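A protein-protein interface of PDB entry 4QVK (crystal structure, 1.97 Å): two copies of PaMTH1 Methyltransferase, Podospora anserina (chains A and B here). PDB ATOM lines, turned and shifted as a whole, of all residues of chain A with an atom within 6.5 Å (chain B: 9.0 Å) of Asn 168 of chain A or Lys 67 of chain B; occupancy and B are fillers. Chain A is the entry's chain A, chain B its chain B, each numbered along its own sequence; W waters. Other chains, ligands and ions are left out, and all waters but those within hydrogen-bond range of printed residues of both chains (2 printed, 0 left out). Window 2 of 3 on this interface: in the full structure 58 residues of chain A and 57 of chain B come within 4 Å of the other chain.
The guanidinium group of Arg 234 of chain A sits close to the side-chain amino group of Lys 67 of chain B, at 3.2 Å. The side-chain amide nitrogen (ND2) of Asn 168 of chain A lies close to the side-chain amino group (NZ) of Lys 67 of chain B, 3.2 Å away. The guanidinium group (NH1) of Arg 66 of chain A lies within salt-bridge range of the side-chain carboxylate (OD2) of Asp 65 of chain B (2.7 Å). The backbone carbonyl oxygen (O) of Arg 64 of chain B sits at hydrogen-bond distance from the guanidinium group (NH2) of Arg 234 of chain A.
O of Arg 64 of chain B lies within hydrogen-bond range of NZ of Lys 67 of chain B, at 2.8 Å. The backbone NH (N) of Ile 170 of chain A lies within hydrogen-bond range of the backbone carbonyl oxygen (O) of Asp 141 of chain A, at 3.2 Å. NH2 of Arg 234 of chain A is in salt-bridge range of OD1 of Asp 237 of chain A.
Among the printed residues, pairs that only touch across the chains: Ile 170 of chain A with Phe 61 of chain B, Arg 234 of chain A with Phe 61 of chain B, Arg 234 of chain A with Asp 65 of chain B and Asp 237 of chain A with Arg 64 of chain B.
Of the printed residues of chain B, Arg 66 of chain A touches Asp 65 (2.7 Å). Printed residues of chain B within 4 Å of Asn 168 of chain A: Lys 67. Of the printed residues of chain A, Phe 61 of chain B touches Ile 170 (3.6 Å) and Arg 234 (3.8 Å). Printed residues of chain A within 4 Å of Arg 64 of chain B: Arg 234 and Asp 237. Of the printed residues of chain A, Asp 65 of chain B touches Arg 66 and Arg 234. Pro 68 of chain B touches none of the printed residues of chain A.
Hydrophobic or aromatic side chains of chain B that line the printed part of chain A: Phe 61. Of the 12 printed residues of chain A, 5 touch a printed residue of chain B. Among the printed residues, 8 pairs touch across the chains.
3 positions are printed for both chains. Of the 8 pairs that touch across the chains among the printed residues, none has its exchanged pair printed and touching as well.
Water W2 lies within hydrogen-bond range of O of Arg 64 of chain B (2.5 Å), OD2 of Asp 237 of chain A (2.8 Å) and NZ of Lys 67 of chain B (3.2 Å). Water W1 lies within hydrogen-bond range of the side-chain carboxylate (OD1) of Asp 65 of chain B, the guanidinium group (NE) of Arg 234 of chain A and the backbone carbonyl oxygen (O) of Gly 169 of chain A.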
ATOM      1  N   ARG A  66     -14.283  -6.261   8.432  1.00  0.00           N
ATOM      2  CA  ARG A  66     -15.054  -7.485   8.625  1.00  0.00           C
ATOM      3  C   ARG A  66     -14.686  -8.591   7.658  1.00  0.00           C
ATOM      4  O   ARG A  66     -14.938  -9.769   7.952  1.00  0.00           O
ATOM      5  CB  ARG A  66     -16.545  -7.189   8.520  1.00  0.00           C
ATOM      6  CG  ARG A  66     -17.023  -6.143   9.537  1.00  0.00           C
ATOM      7  CD  ARG A  66     -18.539  -6.093   9.483  1.00  0.00           C
ATOM      8  NE  ARG A  66     -19.095  -7.324  10.033  1.00  0.00           N
ATOM      9  CZ  ARG A  66     -19.419  -7.470  11.315  1.00  0.00           C
ATOM     10  NH1 ARG A  66     -19.261  -6.452  12.172  1.00  0.00           N
ATOM     11  NH2 ARG A  66     -19.902  -8.628  11.748  1.00  0.00           N
ATOM     12  N   PHE A 140     -25.425 -14.615   4.073  1.00  0.00           N
ATOM     13  CA  PHE A 140     -24.581 -13.445   3.804  1.00  0.00           C
ATOM     14  C   PHE A 140     -23.907 -12.966   5.101  1.00  0.00           C
ATOM     15  O   PHE A 140     -24.511 -13.086   6.178  1.00  0.00           O
ATOM     16  CB  PHE A 140     -25.404 -12.294   3.203  1.00  0.00           C
ATOM     17  CG  PHE A 140     -25.940 -12.568   1.816  1.00  0.00           C
ATOM     18  CD1 PHE A 140     -27.174 -13.195   1.633  1.00  0.00           C
ATOM     19  CD2 PHE A 140     -25.228 -12.179   0.704  1.00  0.00           C
ATOM     20  CE1 PHE A 140     -27.685 -13.439   0.347  1.00  0.00           C
ATOM     21  CE2 PHE A 140     -25.726 -12.425  -0.589  1.00  0.00           C
ATOM     22  CZ  PHE A 140     -26.960 -13.055  -0.758  1.00  0.00           C
ATOM     23  N   ASP A 141     -22.676 -12.457   4.999  1.00  0.00           N
ATOM     24  CA  ASP A 141     -21.891 -12.064   6.169  1.00  0.00           C
ATOM     25  C   ASP A 141     -22.198 -10.635   6.594  1.00  0.00           C
ATOM     26  O   ASP A 141     -21.948 -10.236   7.739  1.00  0.00           O
ATOM     27  CB  ASP A 141     -20.397 -12.151   5.891  1.00  0.00           C
ATOM     28  CG  ASP A 141     -19.913 -13.543   5.689  1.00  0.00           C
ATOM     29  OD1 ASP A 141     -20.536 -14.491   6.219  1.00  0.00           O
ATOM     30  OD2 ASP A 141     -18.859 -13.680   5.025  1.00  0.00           O
ATOM     31  N   LEU A 165     -28.907 -14.493   7.062  1.00  0.00           N
ATOM     32  CA  LEU A 165     -27.813 -13.934   7.857  1.00  0.00           C
ATOM     33  C   LEU A 165     -26.917 -15.059   8.410  1.00  0.00           C
ATOM     34  O   LEU A 165     -27.400 -15.966   9.077  1.00  0.00           O
ATOM     35  CB  LEU A 165     -28.380 -13.077   8.998  1.00  0.00           C
ATOM     36  CG  LEU A 165     -27.400 -12.432   9.989  1.00  0.00           C
ATOM     37  CD1 LEU A 165     -26.543 -11.365   9.314  1.00  0.00           C
ATOM     38  CD2 LEU A 165     -28.163 -11.827  11.163  1.00  0.00           C
ATOM     39  N   SER A 166     -25.622 -15.021   8.118  1.00  0.00           N
ATOM     40  CA  SER A 166     -24.742 -16.075   8.612  1.00  0.00           C
ATOM     41  C   SER A 166     -24.562 -15.950  10.130  1.00  0.00           C
ATOM     42  O   SER A 166     -24.892 -14.911  10.707  1.00  0.00           O
ATOM     43  CB  SER A 166     -23.389 -16.022   7.903  1.00  0.00           C
ATOM     44  OG  SER A 166     -22.654 -14.874   8.299  1.00  0.00           O
ATOM     45  N   ALA A 167     -24.006 -16.986  10.759  1.00  0.00           N
ATOM     46  CA  ALA A 167     -23.868 -17.050  12.226  1.00  0.00           C
ATOM     47  C   ALA A 167     -23.146 -15.857  12.836  1.00  0.00           C
ATOM     48  O   ALA A 167     -23.564 -15.335  13.871  1.00  0.00           O
ATOM     49  CB  ALA A 167     -23.138 -18.351  12.638  1.00  0.00           C
ATOM     50  N   ASN A 168     -22.046 -15.446  12.217  1.00  0.00           N
ATOM     51  CA  ASN A 168     -21.285 -14.312  12.714  1.00  0.00           C
ATOM     52  C   ASN A 168     -21.444 -13.065  11.846  1.00  0.00           C
ATOM     53  O   ASN A 168     -20.554 -12.206  11.784  1.00  0.00           O
ATOM     54  CB  ASN A 168     -19.814 -14.684  12.839  1.00  0.00           C
ATOM     55  CG  ASN A 168     -19.559 -15.637  14.001  1.00  0.00           C
ATOM     56  OD1 ASN A 168     -20.340 -16.571  14.244  1.00  0.00           O
ATOM     57  ND2 ASN A 168     -18.478 -15.384  14.749  1.00  0.00           N
ATOM     58  N   GLY A 169     -22.593 -12.980  11.182  1.00  0.00           N
ATOM     59  CA  GLY A 169     -22.881 -11.846  10.321  1.00  0.00           C
ATOM     60  C   GLY A 169     -23.496 -10.697  11.084  1.00  0.00           C
ATOM     61  O   GLY A 169     -23.761 -10.807  12.271  1.00  0.00           O
ATOM     62  N   ILE A 170     -23.726  -9.589  10.381  1.00  0.00           N
ATOM     63  CA  ILE A 170     -24.410  -8.454  10.940  1.00  0.00           C
ATOM     64  C   ILE A 170     -25.348  -7.870   9.879  1.00  0.00           C
ATOM     65  O   ILE A 170     -25.077  -7.943   8.681  1.00  0.00           O
ATOM     66  CB  ILE A 170     -23.397  -7.408  11.460  1.00  0.00           C
ATOM     67  CG1 ILE A 170     -24.067  -6.401  12.392  1.00  0.00           C
ATOM     68  CG2 ILE A 170     -22.632  -6.723  10.317  1.00  0.00           C
ATOM     69  CD1 ILE A 170     -23.020  -5.623  13.250  1.00  0.00           C
ATOM     70  N   ARG A 234     -27.542  -8.740  15.161  1.00  0.00           N
ATOM     71  CA  ARG A 234     -26.833  -9.994  14.995  1.00  0.00           C
ATOM     72  C   ARG A 234     -27.670 -11.104  15.615  1.00  0.00           C
ATOM     73  O   ARG A 234     -28.570 -10.832  16.411  1.00  0.00           O
ATOM     74  CB  ARG A 234     -25.436  -9.930  15.625  1.00  0.00           C
ATOM     75  CG  ARG A 234     -25.462  -9.719  17.134  1.00  0.00           C
ATOM     76  CD  ARG A 234     -24.059  -9.591  17.696  1.00  0.00           C
ATOM     77  NE  ARG A 234     -23.282 -10.786  17.443  1.00  0.00           N
ATOM     78  CZ  ARG A 234     -23.252 -11.792  18.295  1.00  0.00           C
ATOM     79  NH1 ARG A 234     -23.961 -11.689  19.416  1.00  0.00           N
ATOM     80  NH2 ARG A 234     -22.528 -12.879  18.032  1.00  0.00           N
ATOM     81  N   TRP A 235     -27.401 -12.346  15.230  1.00  0.00           N
ATOM     82  CA  TRP A 235     -27.991 -13.478  15.928  1.00  0.00           C
ATOM     83  C   TRP A 235     -27.546 -13.483  17.384  1.00  0.00           C
ATOM     84  O   TRP A 235     -26.344 -13.430  17.650  1.00  0.00           O
ATOM     85  CB  TRP A 235     -27.572 -14.803  15.294  1.00  0.00           C
ATOM     86  CG  TRP A 235     -28.108 -15.086  13.943  1.00  0.00           C
ATOM     87  CD1 TRP A 235     -27.392 -15.180  12.778  1.00  0.00           C
ATOM     88  CD2 TRP A 235     -29.467 -15.369  13.604  1.00  0.00           C
ATOM     89  NE1 TRP A 235     -28.227 -15.490  11.733  1.00  0.00           N
ATOM     90  CE2 TRP A 235     -29.506 -15.617  12.211  1.00  0.00           C
ATOM     91  CE3 TRP A 235     -30.660 -15.440  14.340  1.00  0.00           C
ATOM     92  CZ2 TRP A 235     -30.700 -15.937  11.535  1.00  0.00           C
ATOM     93  CZ3 TRP A 235     -31.849 -15.743  13.664  1.00  0.00           C
ATOM     94  CH2 TRP A 235     -31.854 -15.990  12.272  1.00  0.00           C
ATOM     95  N   ASP A 237     -26.269 -14.934  20.716  1.00  0.00           N
ATOM     96  CA  ASP A 237     -25.408 -16.111  20.945  1.00  0.00           C
ATOM     97  C   ASP A 237     -26.059 -17.355  21.628  1.00  0.00           C
ATOM     98  O   ASP A 237     -25.837 -18.476  21.159  1.00  0.00           O
ATOM     99  CB  ASP A 237     -24.165 -15.705  21.758  1.00  0.00           C
ATOM    100  CG  ASP A 237     -23.206 -14.819  20.976  1.00  0.00           C
ATOM    101  OD1 ASP A 237     -22.981 -15.081  19.773  1.00  0.00           O
ATOM    102  OD2 ASP A 237     -22.659 -13.873  21.580  1.00  0.00           O
ATOM    103  N   MET B  59     -20.349  -1.348  23.680  1.00  0.00           N
ATOM    104  CA  MET B  59     -19.116  -2.082  23.982  1.00  0.00           C
ATOM    105  C   MET B  59     -19.381  -3.583  24.026  1.00  0.00           C
ATOM    106  O   MET B  59     -18.627  -4.339  23.406  1.00  0.00           O
ATOM    107  CB  MET B  59     -18.480  -1.584  25.289  1.00  0.00           C
ATOM    108  CG  MET B  59     -17.911  -0.204  25.140  1.00  0.00           C
ATOM    109  SD  MET B  59     -17.037   0.346  26.620  1.00  0.00           S
ATOM    110  CE  MET B  59     -18.357   0.696  27.732  1.00  0.00           C
ATOM    111  N   ILE B  60     -20.450  -4.001  24.717  1.00  0.00           N
ATOM    112  CA  ILE B  60     -20.876  -5.401  24.767  1.00  0.00           C
ATOM    113  C   ILE B  60     -21.219  -5.979  23.372  1.00  0.00           C
ATOM    114  O   ILE B  60     -20.724  -7.067  23.007  1.00  0.00           O
ATOM    115  CB  ILE B  60     -22.086  -5.566  25.684  1.00  0.00           C
ATOM    116  CG1 ILE B  60     -21.690  -5.151  27.123  1.00  0.00           C
ATOM    117  CG2 ILE B  60     -22.565  -7.015  25.657  1.00  0.00           C
ATOM    118  CD1 ILE B  60     -22.759  -5.370  28.206  1.00  0.00           C
ATOM    119  N   PHE B  61     -22.042  -5.254  22.602  1.00  0.00           N
ATOM    120  CA  PHE B  61     -22.402  -5.708  21.259  1.00  0.00           C
ATOM    121  C   PHE B  61     -21.122  -5.896  20.434  1.00  0.00           C
ATOM    122  O   PHE B  61     -20.924  -6.925  19.789  1.00  0.00           O
ATOM    123  CB  PHE B  61     -23.347  -4.697  20.562  1.00  0.00           C
ATOM    124  CG  PHE B  61     -23.822  -5.148  19.194  1.00  0.00           C
ATOM    125  CD1 PHE B  61     -22.976  -5.086  18.101  1.00  0.00           C
ATOM    126  CD2 PHE B  61     -25.119  -5.599  19.009  1.00  0.00           C
ATOM    127  CE1 PHE B  61     -23.394  -5.513  16.840  1.00  0.00           C
ATOM    128  CE2 PHE B  61     -25.569  -6.003  17.764  1.00  0.00           C
ATOM    129  CZ  PHE B  61     -24.703  -5.979  16.672  1.00  0.00           C
ATOM    130  N   THR B  62     -20.260  -4.889  20.458  1.00  0.00           N
ATOM    131  CA  THR B  62     -19.006  -4.919  19.723  1.00  0.00           C
ATOM    132  C   THR B  62     -18.151  -6.124  20.081  1.00  0.00           C
ATOM    133  O   THR B  62     -17.589  -6.783  19.194  1.00  0.00           O
ATOM    134  CB  THR B  62     -18.215  -3.625  19.975  1.00  0.00           C
ATOM    135  OG1 THR B  62     -18.987  -2.517  19.478  1.00  0.00           O
ATOM    136  CG2 THR B  62     -16.854  -3.681  19.282  1.00  0.00           C
ATOM    137  N   ALA B  63     -18.050  -6.445  21.373  1.00  0.00           N
ATOM    138  CA  ALA B  63     -17.244  -7.611  21.780  1.00  0.00           C
ATOM    139  C   ALA B  63     -17.896  -8.946  21.369  1.00  0.00           C
ATOM    140  O   ALA B  63     -17.198  -9.891  20.978  1.00  0.00           O
ATOM    141  CB  ALA B  63     -16.991  -7.594  23.291  1.00  0.00           C
ATOM    142  N   ARG B  64     -19.217  -9.030  21.461  1.00  0.00           N
ATOM    143  CA  ARG B  64     -19.918 -10.252  21.067  1.00  0.00           C
ATOM    144  C   ARG B  64     -19.792 -10.521  19.563  1.00  0.00           C
ATOM    145  O   ARG B  64     -19.677 -11.662  19.119  1.00  0.00           O
ATOM    146  CB  ARG B  64     -21.400 -10.166  21.446  1.00  0.00           C
ATOM    147  CG  ARG B  64     -21.681 -10.092  22.948  1.00  0.00           C
ATOM    148  CD  ARG B  64     -23.070 -10.636  23.199  1.00  0.00           C
ATOM    149  NE  ARG B  64     -23.742 -10.109  24.381  1.00  0.00           N
ATOM    150  CZ  ARG B  64     -23.536 -10.566  25.609  1.00  0.00           C
ATOM    151  NH1 ARG B  64     -22.629 -11.523  25.826  1.00  0.00           N
ATOM    152  NH2 ARG B  64     -24.212 -10.048  26.632  1.00  0.00           N
ATOM    153  N   ASP B  65     -19.847  -9.434  18.802  1.00  0.00           N
ATOM    154  CA  ASP B  65     -19.721  -9.444  17.354  1.00  0.00           C
ATOM    155  C   ASP B  65     -18.296  -9.836  16.928  1.00  0.00           C
ATOM    156  O   ASP B  65     -18.091 -10.766  16.154  1.00  0.00           O
ATOM    157  CB  ASP B  65     -20.080  -8.055  16.815  1.00  0.00           C
ATOM    158  CG  ASP B  65     -19.968  -7.968  15.309  1.00  0.00           C
ATOM    159  OD1 ASP B  65     -20.350  -8.916  14.599  1.00  0.00           O
ATOM    160  OD2 ASP B  65     -19.488  -6.930  14.836  1.00  0.00           O
ATOM    161  N   ARG B  66     -17.306  -9.134  17.467  1.00  0.00           N
ATOM    162  CA  ARG B  66     -15.940  -9.229  16.950  1.00  0.00           C
ATOM    163  C   ARG B  66     -15.253 -10.454  17.512  1.00  0.00           C
ATOM    164  O   ARG B  66     -14.292 -10.956  16.919  1.00  0.00           O
ATOM    165  CB  ARG B  66     -15.119  -7.962  17.282  1.00  0.00           C
ATOM    166  CG  ARG B  66     -15.699  -6.633  16.726  1.00  0.00           C
ATOM    167  CD  ARG B  66     -14.668  -5.483  16.865  1.00  0.00           C
ATOM    168  NE  ARG B  66     -13.455  -5.794  16.118  1.00  0.00           N
ATOM    169  CZ  ARG B  66     -13.258  -5.420  14.856  1.00  0.00           C
ATOM    170  NH1 ARG B  66     -14.168  -4.666  14.238  1.00  0.00           N
ATOM    171  NH2 ARG B  66     -12.154  -5.770  14.211  1.00  0.00           N
ATOM    172  N   LYS B  67     -15.733 -10.924  18.659  1.00  0.00           N
ATOM    173  CA  LYS B  67     -15.126 -12.076  19.357  1.00  0.00           C
ATOM    174  C   LYS B  67     -13.605 -12.040  19.439  1.00  0.00           C
ATOM    175  O   LYS B  67     -12.934 -12.968  19.004  1.00  0.00           O
ATOM    176  CB  LYS B  67     -15.545 -13.379  18.692  1.00  0.00           C
ATOM    177  CG  LYS B  67     -17.036 -13.569  18.741  1.00  0.00           C
ATOM    178  CD  LYS B  67     -17.439 -14.856  18.085  1.00  0.00           C
ATOM    179  CE  LYS B  67     -18.948 -14.963  18.002  1.00  0.00           C
ATOM    180  NZ  LYS B  67     -19.617 -13.816  17.271  1.00  0.00           N
ATOM    181  N   PRO B  68     -13.052 -10.976  20.035  1.00  0.00           N
ATOM    182  CA  PRO B  68     -11.606 -10.853  20.131  1.00  0.00           C
ATOM    183  C   PRO B  68     -11.038 -11.862  21.109  1.00  0.00           C
ATOM    184  O   PRO B  68     -11.698 -12.176  22.111  1.00  0.00           O
ATOM    185  CB  PRO B  68     -11.419  -9.416  20.650  1.00  0.00           C
ATOM    186  CG  PRO B  68     -12.635  -9.131  21.426  1.00  0.00           C
ATOM    187  CD  PRO B  68     -13.748  -9.895  20.757  1.00  0.00           C
ATOM    188  N   LYS B  69      -9.835 -12.361  20.829  1.00  0.00           N
ATOM    189  CA  LYS B  69      -9.203 -13.329  21.702  1.00  0.00           C
ATOM    190  C   LYS B  69      -8.642 -12.646  22.960  1.00  0.00           C
ATOM    191  O   LYS B  69      -8.653 -13.239  24.040  1.00  0.00           O
ATOM    192  CB  LYS B  69      -8.101 -14.090  20.949  1.00  0.00           C
ATOM    193  CG  LYS B  69      -7.275 -14.998  21.847  1.00  0.00           C
ATOM    194  CD  LYS B  69      -6.334 -15.922  21.083  1.00  0.00           C
ATOM    195  CE  LYS B  69      -5.416 -16.657  22.076  1.00  0.00           C
ATOM    196  NZ  LYS B  69      -4.487 -15.668  22.773  1.00  0.00           N
ATOM    197  N   ARG B  70      -8.165 -11.405  22.799  1.00  0.00           N
ATOM    198  CA  ARG B  70      -7.594 -10.579  23.876  1.00  0.00           C
ATOM    199  C   ARG B  70      -7.950  -9.133  23.622  1.00  0.00           C
ATOM    200  O   ARG B  70      -7.886  -8.670  22.462  1.00  0.00           O
ATOM    201  CB  ARG B  70      -6.062 -10.630  23.959  1.00  0.00           C
ATOM    202  CG  ARG B  70      -5.405 -11.887  24.349  1.00  0.00           C
ATOM    203  CD  ARG B  70      -3.903 -11.675  24.261  1.00  0.00           C
ATOM    204  NE  ARG B  70      -3.240 -11.179  25.477  1.00  0.00           N
ATOM    205  CZ  ARG B  70      -2.121 -10.448  25.474  1.00  0.00           C
ATOM    206  NH1 ARG B  70      -1.551 -10.085  24.325  1.00  0.00           N
ATOM    207  NH2 ARG B  70      -1.575 -10.062  26.619  1.00  0.00           N
ATOM    208  N   ILE B  71      -8.235  -8.420  24.711  1.00  0.00           N
ATOM    209  CA  ILE B  71      -8.574  -7.000  24.671  1.00  0.00           C
ATOM    210  C   ILE B  71      -7.612  -6.179  25.531  1.00  0.00           C
ATOM    211  O   ILE B  71      -7.248  -6.592  26.643  1.00  0.00           O
ATOM    212  CB  ILE B  71     -10.004  -6.772  25.179  1.00  0.00           C
ATOM    213  CG1 ILE B  71     -10.998  -7.485  24.260  1.00  0.00           C
ATOM    214  CG2 ILE B  71     -10.323  -5.309  25.301  1.00  0.00           C
ATOM    215  CD1 ILE B  71     -12.407  -7.404  24.804  1.00  0.00           C
ATOM    216  N   GLY B  88     -19.184  -9.080  27.374  1.00  0.00           N
ATOM    217  CA  GLY B  88     -19.306  -9.403  25.968  1.00  0.00           C
ATOM    218  C   GLY B  88     -18.354 -10.514  25.552  1.00  0.00           C
ATOM    219  O   GLY B  88     -18.416 -10.964  24.418  1.00  0.00           O
ATOM    220  N   THR B  89     -17.461 -10.956  26.441  1.00  0.00           N
ATOM    221  CA  THR B  89     -16.548 -12.030  26.041  1.00  0.00           C
ATOM    222  C   THR B  89     -16.668 -13.260  26.942  1.00  0.00           C
ATOM    223  O   THR B  89     -15.724 -14.024  27.074  1.00  0.00           O
ATOM    224  CB  THR B  89     -15.079 -11.561  26.043  1.00  0.00           C
ATOM    225  OG1 THR B  89     -14.771 -11.038  27.331  1.00  0.00           O
ATOM    226  CG2 THR B  89     -14.826 -10.492  24.987  1.00  0.00           C
ATOM    227  N   ARG B  90     -17.826 -13.426  27.571  1.00  0.00           N
ATOM    228  CA  ARG B  90     -18.065 -14.528  28.501  1.00  0.00           C
ATOM    229  C   ARG B  90     -17.855 -15.921  27.923  1.00  0.00           C
ATOM    230  O   ARG B  90     -17.327 -16.798  28.587  1.00  0.00           O
ATOM    231  CB  ARG B  90     -19.485 -14.451  29.054  1.00  0.00           C
ATOM    232  CG  ARG B  90     -19.648 -13.477  30.176  1.00  0.00           C
ATOM    233  CD  ARG B  90     -21.013 -13.602  30.787  1.00  0.00           C
ATOM    234  NE  ARG B  90     -21.126 -12.706  31.931  1.00  0.00           N
ATOM    235  CZ  ARG B  90     -20.786 -13.021  33.176  1.00  0.00           C
ATOM    236  NH1 ARG B  90     -20.327 -14.237  33.462  1.00  0.00           N
ATOM    237  NH2 ARG B  90     -20.918 -12.118  34.141  1.00  0.00           N
ATOM    238  N   ASP B  91     -18.279 -16.159  26.696  1.00  0.00           N
ATOM    239  CA  ASP B  91     -18.197 -17.527  26.222  1.00  0.00           C
ATOM    240  C   ASP B  91     -16.904 -17.823  25.490  1.00  0.00           C
ATOM    241  O   ASP B  91     -16.695 -18.940  25.032  1.00  0.00           O
ATOM    242  CB  ASP B  91     -19.400 -17.863  25.348  1.00  0.00           C
ATOM    243  CG  ASP B  91     -20.716 -17.507  26.015  1.00  0.00           C
ATOM    244  OD1 ASP B  91     -20.774 -17.553  27.266  1.00  0.00           O
ATOM    245  OD2 ASP B  91     -21.698 -17.220  25.295  1.00  0.00           O
ATOM    246  N   THR B  92     -16.020 -16.842  25.403  1.00  0.00           N
ATOM    247  CA  THR B  92     -14.718 -17.091  24.812  1.00  0.00           C
ATOM    248  C   THR B  92     -13.585 -16.947  25.798  1.00  0.00           C
ATOM    249  O   THR B  92     -12.419 -17.126  25.430  1.00  0.00           O
ATOM    250  CB  THR B  92     -14.414 -16.148  23.701  1.00  0.00           C
ATOM    251  OG1 THR B  92     -14.051 -14.889  24.280  1.00  0.00           O
ATOM    252  CG2 THR B  92     -15.614 -16.008  22.807  1.00  0.00           C
ATOM    253  N   LYS B  93     -13.915 -16.561  27.023  1.00  0.00           N
ATOM    254  CA  LYS B  93     -12.907 -16.475  28.048  1.00  0.00           C
ATOM    255  C   LYS B  93     -11.749 -15.528  27.683  1.00  0.00           C
ATOM    256  O   LYS B  93     -10.620 -15.767  28.107  1.00  0.00           O
ATOM    257  CB  LYS B  93     -12.337 -17.864  28.312  1.00  0.00           C
ATOM    258  CG  LYS B  93     -13.330 -18.927  28.688  1.00  0.00           C
ATOM    259  CD  LYS B  93     -12.590 -20.256  28.734  1.00  0.00           C
ATOM    260  CE  LYS B  93     -13.442 -21.429  29.152  1.00  0.00           C
ATOM    261  NZ  LYS B  93     -12.541 -22.571  29.468  1.00  0.00           N
ATOM    262  N   ALA B  94     -12.008 -14.482  26.900  1.00  0.00           N
ATOM    263  CA  ALA B  94     -10.956 -13.542  26.490  1.00  0.00           C
ATOM    264  C   ALA B  94     -10.202 -12.887  27.659  1.00  0.00           C
ATOM    265  O   ALA B  94     -10.822 -12.461  28.632  1.00  0.00           O
ATOM    266  CB  ALA B  94     -11.545 -12.455  25.626  1.00  0.00           C
ATOM    267  N   ASP B 141      -6.754  -8.160  19.829  1.00  0.00           N
ATOM    268  CA  ASP B 141      -7.674  -8.126  18.713  1.00  0.00           C
ATOM    269  C   ASP B 141      -8.539  -6.864  18.775  1.00  0.00           C
ATOM    270  O   ASP B 141      -9.150  -6.450  17.794  1.00  0.00           O
ATOM    271  CB  ASP B 141      -8.572  -9.356  18.734  1.00  0.00           C
ATOM    272  CG  ASP B 141      -7.910 -10.599  18.165  1.00  0.00           C
ATOM    273  OD1 ASP B 141      -7.013 -10.453  17.302  1.00  0.00           O
ATOM    274  OD2 ASP B 141      -8.332 -11.725  18.550  1.00  0.00           O
ATOM    275  N   LEU B 142      -8.614  -6.278  19.962  1.00  0.00           N
ATOM    276  CA  LEU B 142      -9.422  -5.094  20.173  1.00  0.00           C
ATOM    277  C   LEU B 142      -8.701  -4.252  21.229  1.00  0.00           C
ATOM    278  O   LEU B 142      -8.327  -4.760  22.309  1.00  0.00           O
ATOM    279  CB  LEU B 142     -10.839  -5.482  20.604  1.00  0.00           C
ATOM    280  CG  LEU B 142     -11.820  -4.377  21.022  1.00  0.00           C
ATOM    281  CD1 LEU B 142     -12.060  -3.497  19.865  1.00  0.00           C
ATOM    282  CD2 LEU B 142     -13.147  -5.018  21.456  1.00  0.00           C
ATOM    283  N   ASN B 168      -5.804  -8.671  12.164  1.00  0.00           N
ATOM    284  CA  ASN B 168      -7.227  -8.394  11.928  1.00  0.00           C
ATOM    285  C   ASN B 168      -7.898  -7.549  13.027  1.00  0.00           C
ATOM    286  O   ASN B 168      -9.108  -7.436  13.076  1.00  0.00           O
ATOM    287  CB  ASN B 168      -7.995  -9.696  11.748  1.00  0.00           C
ATOM    288  CG  ASN B 168      -7.613 -10.430  10.469  1.00  0.00           C
ATOM    289  OD1 ASN B 168      -7.021  -9.849   9.556  1.00  0.00           O
ATOM    290  ND2 ASN B 168      -7.992 -11.691  10.378  1.00  0.00           N
HETATM  291  O   HOH W   1     -22.096 -10.746  14.791  1.00  0.00           O
HETATM  292  O   HOH W   2     -20.076 -13.799  20.405  1.00  0.00           O
